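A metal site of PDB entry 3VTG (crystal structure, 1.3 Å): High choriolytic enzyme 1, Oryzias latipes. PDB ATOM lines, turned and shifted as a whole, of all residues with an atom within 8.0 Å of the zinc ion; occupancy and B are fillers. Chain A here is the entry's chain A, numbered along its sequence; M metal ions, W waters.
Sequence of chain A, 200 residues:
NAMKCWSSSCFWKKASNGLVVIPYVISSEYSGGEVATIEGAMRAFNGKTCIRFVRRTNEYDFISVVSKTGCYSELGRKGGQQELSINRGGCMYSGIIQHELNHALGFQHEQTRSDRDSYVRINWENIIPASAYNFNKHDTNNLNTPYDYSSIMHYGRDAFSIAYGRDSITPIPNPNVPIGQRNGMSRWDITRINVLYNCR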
ATOM      1  N   CYS A  71      -1.749  19.111  18.131  1.00  0.00           N
ATOM      2  CA  CYS A  71      -0.529  19.910  17.996  1.00  0.00           C
ATOM      3  C   CYS A  71       0.509  19.071  17.259  1.00  0.00           C
ATOM      4  O   CYS A  71       0.925  18.021  17.745  1.00  0.00           O
ATOM      5  CB  CYS A  71       0.012  20.317  19.369  1.00  0.00           C
ATOM      6  SG  CYS A  71      -1.188  20.441  20.730  1.00  0.00           S
ATOM      7  N   TYR A  72       0.912  19.520  16.071  1.00  0.00           N
ATOM      8  CA  TYR A  72       1.888  18.787  15.263  1.00  0.00           C
ATOM      9  C   TYR A  72       2.654  19.684  14.294  1.00  0.00           C
ATOM     10  O   TYR A  72       2.260  20.810  14.015  1.00  0.00           O
ATOM     11  CB  TYR A  72       1.249  17.598  14.537  1.00  0.00           C
ATOM     12  CG  TYR A  72       0.242  17.942  13.452  1.00  0.00           C
ATOM     13  CD1 TYR A  72      -1.122  17.774  13.672  1.00  0.00           C
ATOM     14  CD2 TYR A  72       0.657  18.397  12.197  1.00  0.00           C
ATOM     15  CE1 TYR A  72      -2.053  18.071  12.682  1.00  0.00           C
ATOM     16  CE2 TYR A  72      -0.261  18.701  11.207  1.00  0.00           C
ATOM     17  CZ  TYR A  72      -1.611  18.537  11.451  1.00  0.00           C
ATOM     18  OH  TYR A  72      -2.525  18.834  10.476  1.00  0.00           O
ATOM     19  N   SER A  73       3.753  19.150  13.787  1.00  0.00           N
ATOM     20  CA  SER A  73       4.551  19.822  12.778  1.00  0.00           C
ATOM     21  C   SER A  73       5.275  18.789  11.926  1.00  0.00           C
ATOM     22  O   SER A  73       5.548  17.675  12.382  1.00  0.00           O
ATOM     23  CB  SER A  73       5.580  20.746  13.423  1.00  0.00           C
ATOM     24  OG  SER A  73       6.441  21.308  12.442  1.00  0.00           O
ATOM     25  N   ILE A  96       4.114  24.347  24.401  1.00  0.00           N
ATOM     26  CA  ILE A  96       3.646  23.451  23.345  1.00  0.00           C
ATOM     27  C   ILE A  96       4.007  24.013  21.964  1.00  0.00           C
ATOM     28  O   ILE A  96       4.489  23.271  21.084  1.00  0.00           O
ATOM     29  CB  ILE A  96       2.125  23.186  23.457  1.00  0.00           C
ATOM     30  CG1 ILE A  96       1.844  22.330  24.705  1.00  0.00           C
ATOM     31  CG2 ILE A  96       1.596  22.507  22.203  1.00  0.00           C
ATOM     32  CD1 ILE A  96       0.369  22.099  24.992  1.00  0.00           C
ATOM     33  N   HIS A  99       7.676  23.558  21.402  1.00  0.00           N
ATOM     34  CA  HIS A  99       7.863  22.131  21.080  1.00  0.00           C
ATOM     35  C   HIS A  99       7.620  21.902  19.602  1.00  0.00           C
ATOM     36  O   HIS A  99       8.458  21.281  18.924  1.00  0.00           O
ATOM     37  CB  HIS A  99       6.919  21.317  21.959  1.00  0.00           C
ATOM     38  CG  HIS A  99       6.869  19.834  21.637  1.00  0.00           C
ATOM     39  ND1 HIS A  99       7.408  18.899  22.438  1.00  0.00           N
ATOM     40  CD2 HIS A  99       6.275  19.156  20.579  1.00  0.00           C
ATOM     41  CE1 HIS A  99       7.189  17.679  21.917  1.00  0.00           C
ATOM     42  NE2 HIS A  99       6.494  17.835  20.776  1.00  0.00           N
ATOM     43  N   GLU A 100       6.516  22.419  19.078  1.00  0.00           N
ATOM     44  CA  GLU A 100       6.190  22.246  17.656  1.00  0.00           C
ATOM     45  C   GLU A 100       7.189  22.939  16.731  1.00  0.00           C
ATOM     46  O   GLU A 100       7.577  22.372  15.697  1.00  0.00           O
ATOM     47  CB  GLU A 100       4.756  22.714  17.351  1.00  0.00           C
ATOM     48  CG  GLU A 100       3.659  21.936  18.065  1.00  0.00           C
ATOM     49  CD  GLU A 100       3.768  20.435  17.901  1.00  0.00           C
ATOM     50  OE1 GLU A 100       4.298  19.948  16.878  1.00  0.00           O
ATOM     51  OE2 GLU A 100       3.323  19.718  18.826  1.00  0.00           O
ATOM     52  N   ASN A 102      10.273  23.435  17.391  1.00  0.00           N
ATOM     53  CA  ASN A 102      11.456  22.566  17.428  1.00  0.00           C
ATOM     54  C   ASN A 102      11.374  21.386  16.455  1.00  0.00           C
ATOM     55  O   ASN A 102      12.380  21.012  15.845  1.00  0.00           O
ATOM     56  CB  ASN A 102      11.756  22.090  18.844  1.00  0.00           C
ATOM     57  CG  ASN A 102      12.696  23.028  19.573  1.00  0.00           C
ATOM     58  OD1 ASN A 102      13.899  23.052  19.298  1.00  0.00           O
ATOM     59  ND2 ASN A 102      12.145  23.818  20.493  1.00  0.00           N
ATOM     60  N   HIS A 103      10.178  20.797  16.294  1.00  0.00           N
ATOM     61  CA  HIS A 103       9.965  19.799  15.244  1.00  0.00           C
ATOM     62  C   HIS A 103      10.275  20.378  13.899  1.00  0.00           C
ATOM     63  O   HIS A 103      10.985  19.767  13.096  1.00  0.00           O
ATOM     64  CB  HIS A 103       8.538  19.272  15.235  1.00  0.00           C
ATOM     65  CG  HIS A 103       8.224  18.245  16.314  1.00  0.00           C
ATOM     66  ND1 HIS A 103       9.032  17.208  16.600  1.00  0.00           N
ATOM     67  CD2 HIS A 103       7.108  18.106  17.128  1.00  0.00           C
ATOM     68  CE1 HIS A 103       8.468  16.456  17.567  1.00  0.00           C
ATOM     69  NE2 HIS A 103       7.293  17.006  17.892  1.00  0.00           N
ATOM     70  N   PHE A 107      13.966  18.535  15.022  1.00  0.00           N
ATOM     71  CA  PHE A 107      14.145  17.746  16.253  1.00  0.00           C
ATOM     72  C   PHE A 107      12.991  16.807  16.554  1.00  0.00           C
ATOM     73  O   PHE A 107      11.813  17.145  16.367  1.00  0.00           O
ATOM     74  CB  PHE A 107      14.425  18.671  17.440  1.00  0.00           C
ATOM     75  CG  PHE A 107      15.713  19.422  17.296  1.00  0.00           C
ATOM     76  CD1 PHE A 107      16.930  18.779  17.501  1.00  0.00           C
ATOM     77  CD2 PHE A 107      15.706  20.756  16.922  1.00  0.00           C
ATOM     78  CE1 PHE A 107      18.122  19.469  17.349  1.00  0.00           C
ATOM     79  CE2 PHE A 107      16.899  21.447  16.770  1.00  0.00           C
ATOM     80  CZ  PHE A 107      18.101  20.800  16.984  1.00  0.00           C
ATOM     81  N   GLN A 108      13.342  15.615  17.018  1.00  0.00           N
ATOM     82  CA  GLN A 108      12.381  14.554  17.308  1.00  0.00           C
ATOM     83  C   GLN A 108      12.199  14.377  18.812  1.00  0.00           C
ATOM     84  O   GLN A 108      12.929  14.973  19.604  1.00  0.00           O
ATOM     85  CB  GLN A 108      12.836  13.256  16.650  1.00  0.00           C
ATOM     86  CG  GLN A 108      13.074  13.408  15.158  1.00  0.00           C
ATOM     87  CD  GLN A 108      13.713  12.200  14.518  1.00  0.00           C
ATOM     88  OE1 GLN A 108      14.932  12.154  14.343  1.00  0.00           O
ATOM     89  NE2 GLN A 108      12.897  11.207  14.188  1.00  0.00           N
ATOM     90  N   HIS A 109      11.215  13.568  19.199  1.00  0.00           N
ATOM     91  CA  HIS A 109      10.951  13.320  20.614  1.00  0.00           C
ATOM     92  C   HIS A 109      12.104  12.662  21.289  1.00  0.00           C
ATOM     93  O   HIS A 109      12.732  11.743  20.734  1.00  0.00           O
ATOM     94  CB  HIS A 109       9.681  12.494  20.783  1.00  0.00           C
ATOM     95  CG  HIS A 109       8.430  13.195  20.300  1.00  0.00           C
ATOM     96  ND1 HIS A 109       7.528  12.600  19.510  1.00  0.00           N
ATOM     97  CD2 HIS A 109       7.986  14.499  20.511  1.00  0.00           C
ATOM     98  CE1 HIS A 109       6.545  13.474  19.230  1.00  0.00           C
ATOM     99  NE2 HIS A 109       6.826  14.631  19.849  1.00  0.00           N
ATOM    100  N   GLU A 110      12.411  13.132  22.500  1.00  0.00           N
ATOM    101  CA  GLU A 110      13.566  12.657  23.254  1.00  0.00           C
ATOM    102  C   GLU A 110      13.577  11.145  23.472  1.00  0.00           C
ATOM    103  O   GLU A 110      14.638  10.513  23.344  1.00  0.00           O
ATOM    104  CB  GLU A 110      13.668  13.396  24.600  1.00  0.00           C
ATOM    105  CG  GLU A 110      15.004  13.257  25.309  1.00  0.00           C
ATOM    106  CD  GLU A 110      16.123  14.042  24.630  1.00  0.00           C
ATOM    107  OE1 GLU A 110      15.903  14.648  23.569  1.00  0.00           O
ATOM    108  OE2 GLU A 110      17.248  14.038  25.185  1.00  0.00           O
ATOM    109  N   GLN A 111      12.415  10.574  23.770  1.00  0.00           N
ATOM    110  CA  GLN A 111      12.327   9.149  24.082  1.00  0.00           C
ATOM    111  C   GLN A 111      12.603   8.238  22.879  1.00  0.00           C
ATOM    112  O   GLN A 111      12.711   7.024  23.026  1.00  0.00           O
ATOM    113  CB  GLN A 111      10.975   8.795  24.731  1.00  0.00           C
ATOM    114  CG  GLN A 111       9.789   8.688  23.774  1.00  0.00           C
ATOM    115  CD  GLN A 111       9.153  10.021  23.447  1.00  0.00           C
ATOM    116  OE1 GLN A 111       9.464  11.055  24.060  1.00  0.00           O
ATOM    117  NE2 GLN A 111       8.264  10.022  22.472  1.00  0.00           N
ATOM    118  N   ASN A 134       4.737   6.122  18.215  1.00  0.00           N
ATOM    119  CA  ASN A 134       5.339   7.345  18.750  1.00  0.00           C
ATOM    120  C   ASN A 134       6.502   7.069  19.699  1.00  0.00           C
ATOM    121  O   ASN A 134       7.239   7.986  20.087  1.00  0.00           O
ATOM    122  CB  ASN A 134       4.294   8.182  19.474  1.00  0.00           C
ATOM    123  CG  ASN A 134       3.222   8.724  18.545  1.00  0.00           C
ATOM    124  OD1 ASN A 134       3.499   9.549  17.678  1.00  0.00           O
ATOM    125  ND2 ASN A 134       1.990   8.272  18.741  1.00  0.00           N
ATOM    126  N   ILE A 152      12.188  19.745  26.384  1.00  0.00           N
ATOM    127  CA  ILE A 152      10.834  20.117  25.972  1.00  0.00           C
ATOM    128  C   ILE A 152      10.277  19.108  24.954  1.00  0.00           C
ATOM    129  O   ILE A 152       9.087  19.126  24.634  1.00  0.00           O
ATOM    130  CB  ILE A 152      10.800  21.566  25.429  1.00  0.00           C
ATOM    131  CG1 ILE A 152       9.403  22.187  25.592  1.00  0.00           C
ATOM    132  CG2 ILE A 152      11.312  21.626  23.989  1.00  0.00           C
ATOM    133  CD1 ILE A 152       9.338  23.663  25.253  1.00  0.00           C
ATOM    134  N   MET A 153      11.143  18.229  24.450  1.00  0.00           N
ATOM    135  CA  MET A 153      10.767  17.218  23.466  1.00  0.00           C
ATOM    136  C   MET A 153      10.463  15.845  24.072  1.00  0.00           C
ATOM    137  O   MET A 153      10.123  14.902  23.346  1.00  0.00           O
ATOM    138  CB  MET A 153      11.849  17.076  22.385  1.00  0.00           C
ATOM    139  CG  MET A 153      12.231  18.382  21.693  1.00  0.00           C
ATOM    140  SD  MET A 153      10.837  19.327  21.047  1.00  0.00           S
ATOM    141  CE  MET A 153      10.345  18.302  19.662  1.00  0.00           C
ATOM    142  N   HIS A 154      10.598  15.710  25.390  1.00  0.00           N
ATOM    143  CA  HIS A 154      10.350  14.439  26.055  1.00  0.00           C
ATOM    144  C   HIS A 154       8.903  14.275  26.397  1.00  0.00           C
ATOM    145  O   HIS A 154       8.305  15.157  26.999  1.00  0.00           O
ATOM    146  CB  HIS A 154      11.196  14.333  27.321  1.00  0.00           C
ATOM    147  CG  HIS A 154      11.487  12.904  27.750  1.00  0.00           C
ATOM    148  ND1 HIS A 154      10.523  12.019  28.064  1.00  0.00           N
ATOM    149  CD2 HIS A 154      12.697  12.229  27.890  1.00  0.00           C
ATOM    150  CE1 HIS A 154      11.083  10.845  28.393  1.00  0.00           C
ATOM    151  NE2 HIS A 154      12.414  10.973  28.283  1.00  0.00           N
ATOM    152  N   TYR A 155       8.319  13.135  26.021  1.00  0.00           N
ATOM    153  CA  TYR A 155       6.972  12.770  26.452  1.00  0.00           C
ATOM    154  C   TYR A 155       6.883  12.657  27.974  1.00  0.00           C
ATOM    155  O   TYR A 155       7.850  12.266  28.634  1.00  0.00           O
ATOM    156  CB  TYR A 155       6.584  11.403  25.864  1.00  0.00           C
ATOM    157  CG  TYR A 155       5.980  11.388  24.474  1.00  0.00           C
ATOM    158  CD1 TYR A 155       6.007  12.502  23.633  1.00  0.00           C
ATOM    159  CD2 TYR A 155       5.390  10.215  23.999  1.00  0.00           C
ATOM    160  CE1 TYR A 155       5.454  12.442  22.353  1.00  0.00           C
ATOM    161  CE2 TYR A 155       4.841  10.148  22.734  1.00  0.00           C
ATOM    162  CZ  TYR A 155       4.871  11.259  21.917  1.00  0.00           C
ATOM    163  OH  TYR A 155       4.316  11.186  20.664  1.00  0.00           O
ATOM    164  N   ARG A 182       6.618  21.211  29.773  1.00  0.00           N
ATOM    165  CA  ARG A 182       6.351  22.082  28.631  1.00  0.00           C
ATOM    166  C   ARG A 182       6.383  23.555  29.065  1.00  0.00           C
ATOM    167  O   ARG A 182       5.587  24.372  28.608  1.00  0.00           O
ATOM    168  CB  ARG A 182       5.037  21.719  27.931  1.00  0.00           C
ATOM    169  CG  ARG A 182       5.017  20.338  27.294  1.00  0.00           C
ATOM    170  CD  ARG A 182       6.005  20.201  26.143  1.00  0.00           C
ATOM    171  NE  ARG A 182       5.926  18.878  25.522  1.00  0.00           N
ATOM    172  CZ  ARG A 182       6.635  17.815  25.895  1.00  0.00           C
ATOM    173  NH1 ARG A 182       7.498  17.901  26.905  1.00  0.00           N
ATOM    174  NH2 ARG A 182       6.498  16.662  25.265  1.00  0.00           N
HETATM  175 ZN    ZN M   1       5.940  16.409  19.392  1.00  0.00          ZN
HETATM  176  O   HOH W   1       4.264  17.217  18.347  1.00  0.00           O
HETATM  177  O   HOH W   2       4.209  15.800  20.794  1.00  0.00           O
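Three residues have an atom within 4 Å of the zinc ion: His 99, His 103 and His 109.
The zinc ion is bound by NE2 of His 109 (2.0 Å).
The zinc ion is bound by NE2 of His 99, at 2.1 Å.
A ring nitrogen (NE2) of His 103 binds the zinc ion (2.1 Å).
Water W1 binds the zinc ion (2.1 Å).
The zinc ion is bound by water W2 (2.3 Å).
Water W1 lies within hydrogen-bond range of OE2 of Glu 100 and O of Cys 71.
A ring nitrogen (ND1) of His 99 sits at hydrogen-bond distance from the side-chain sulfur (SD) of Met 153 (3.7 Å).
ND1 of His 99 is in hydrogen-bond range of NE of Arg 182 (3.4 Å).
A ring nitrogen (ND1) of His 99 sits at hydrogen-bond distance from the backbone carbonyl oxygen (O) of Ile 152, at 2.8 Å.
A ring nitrogen (ND1) of His 103 sits at hydrogen-bond distance from the backbone carbonyl oxygen (O) of Phe 107 (2.8 Å).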
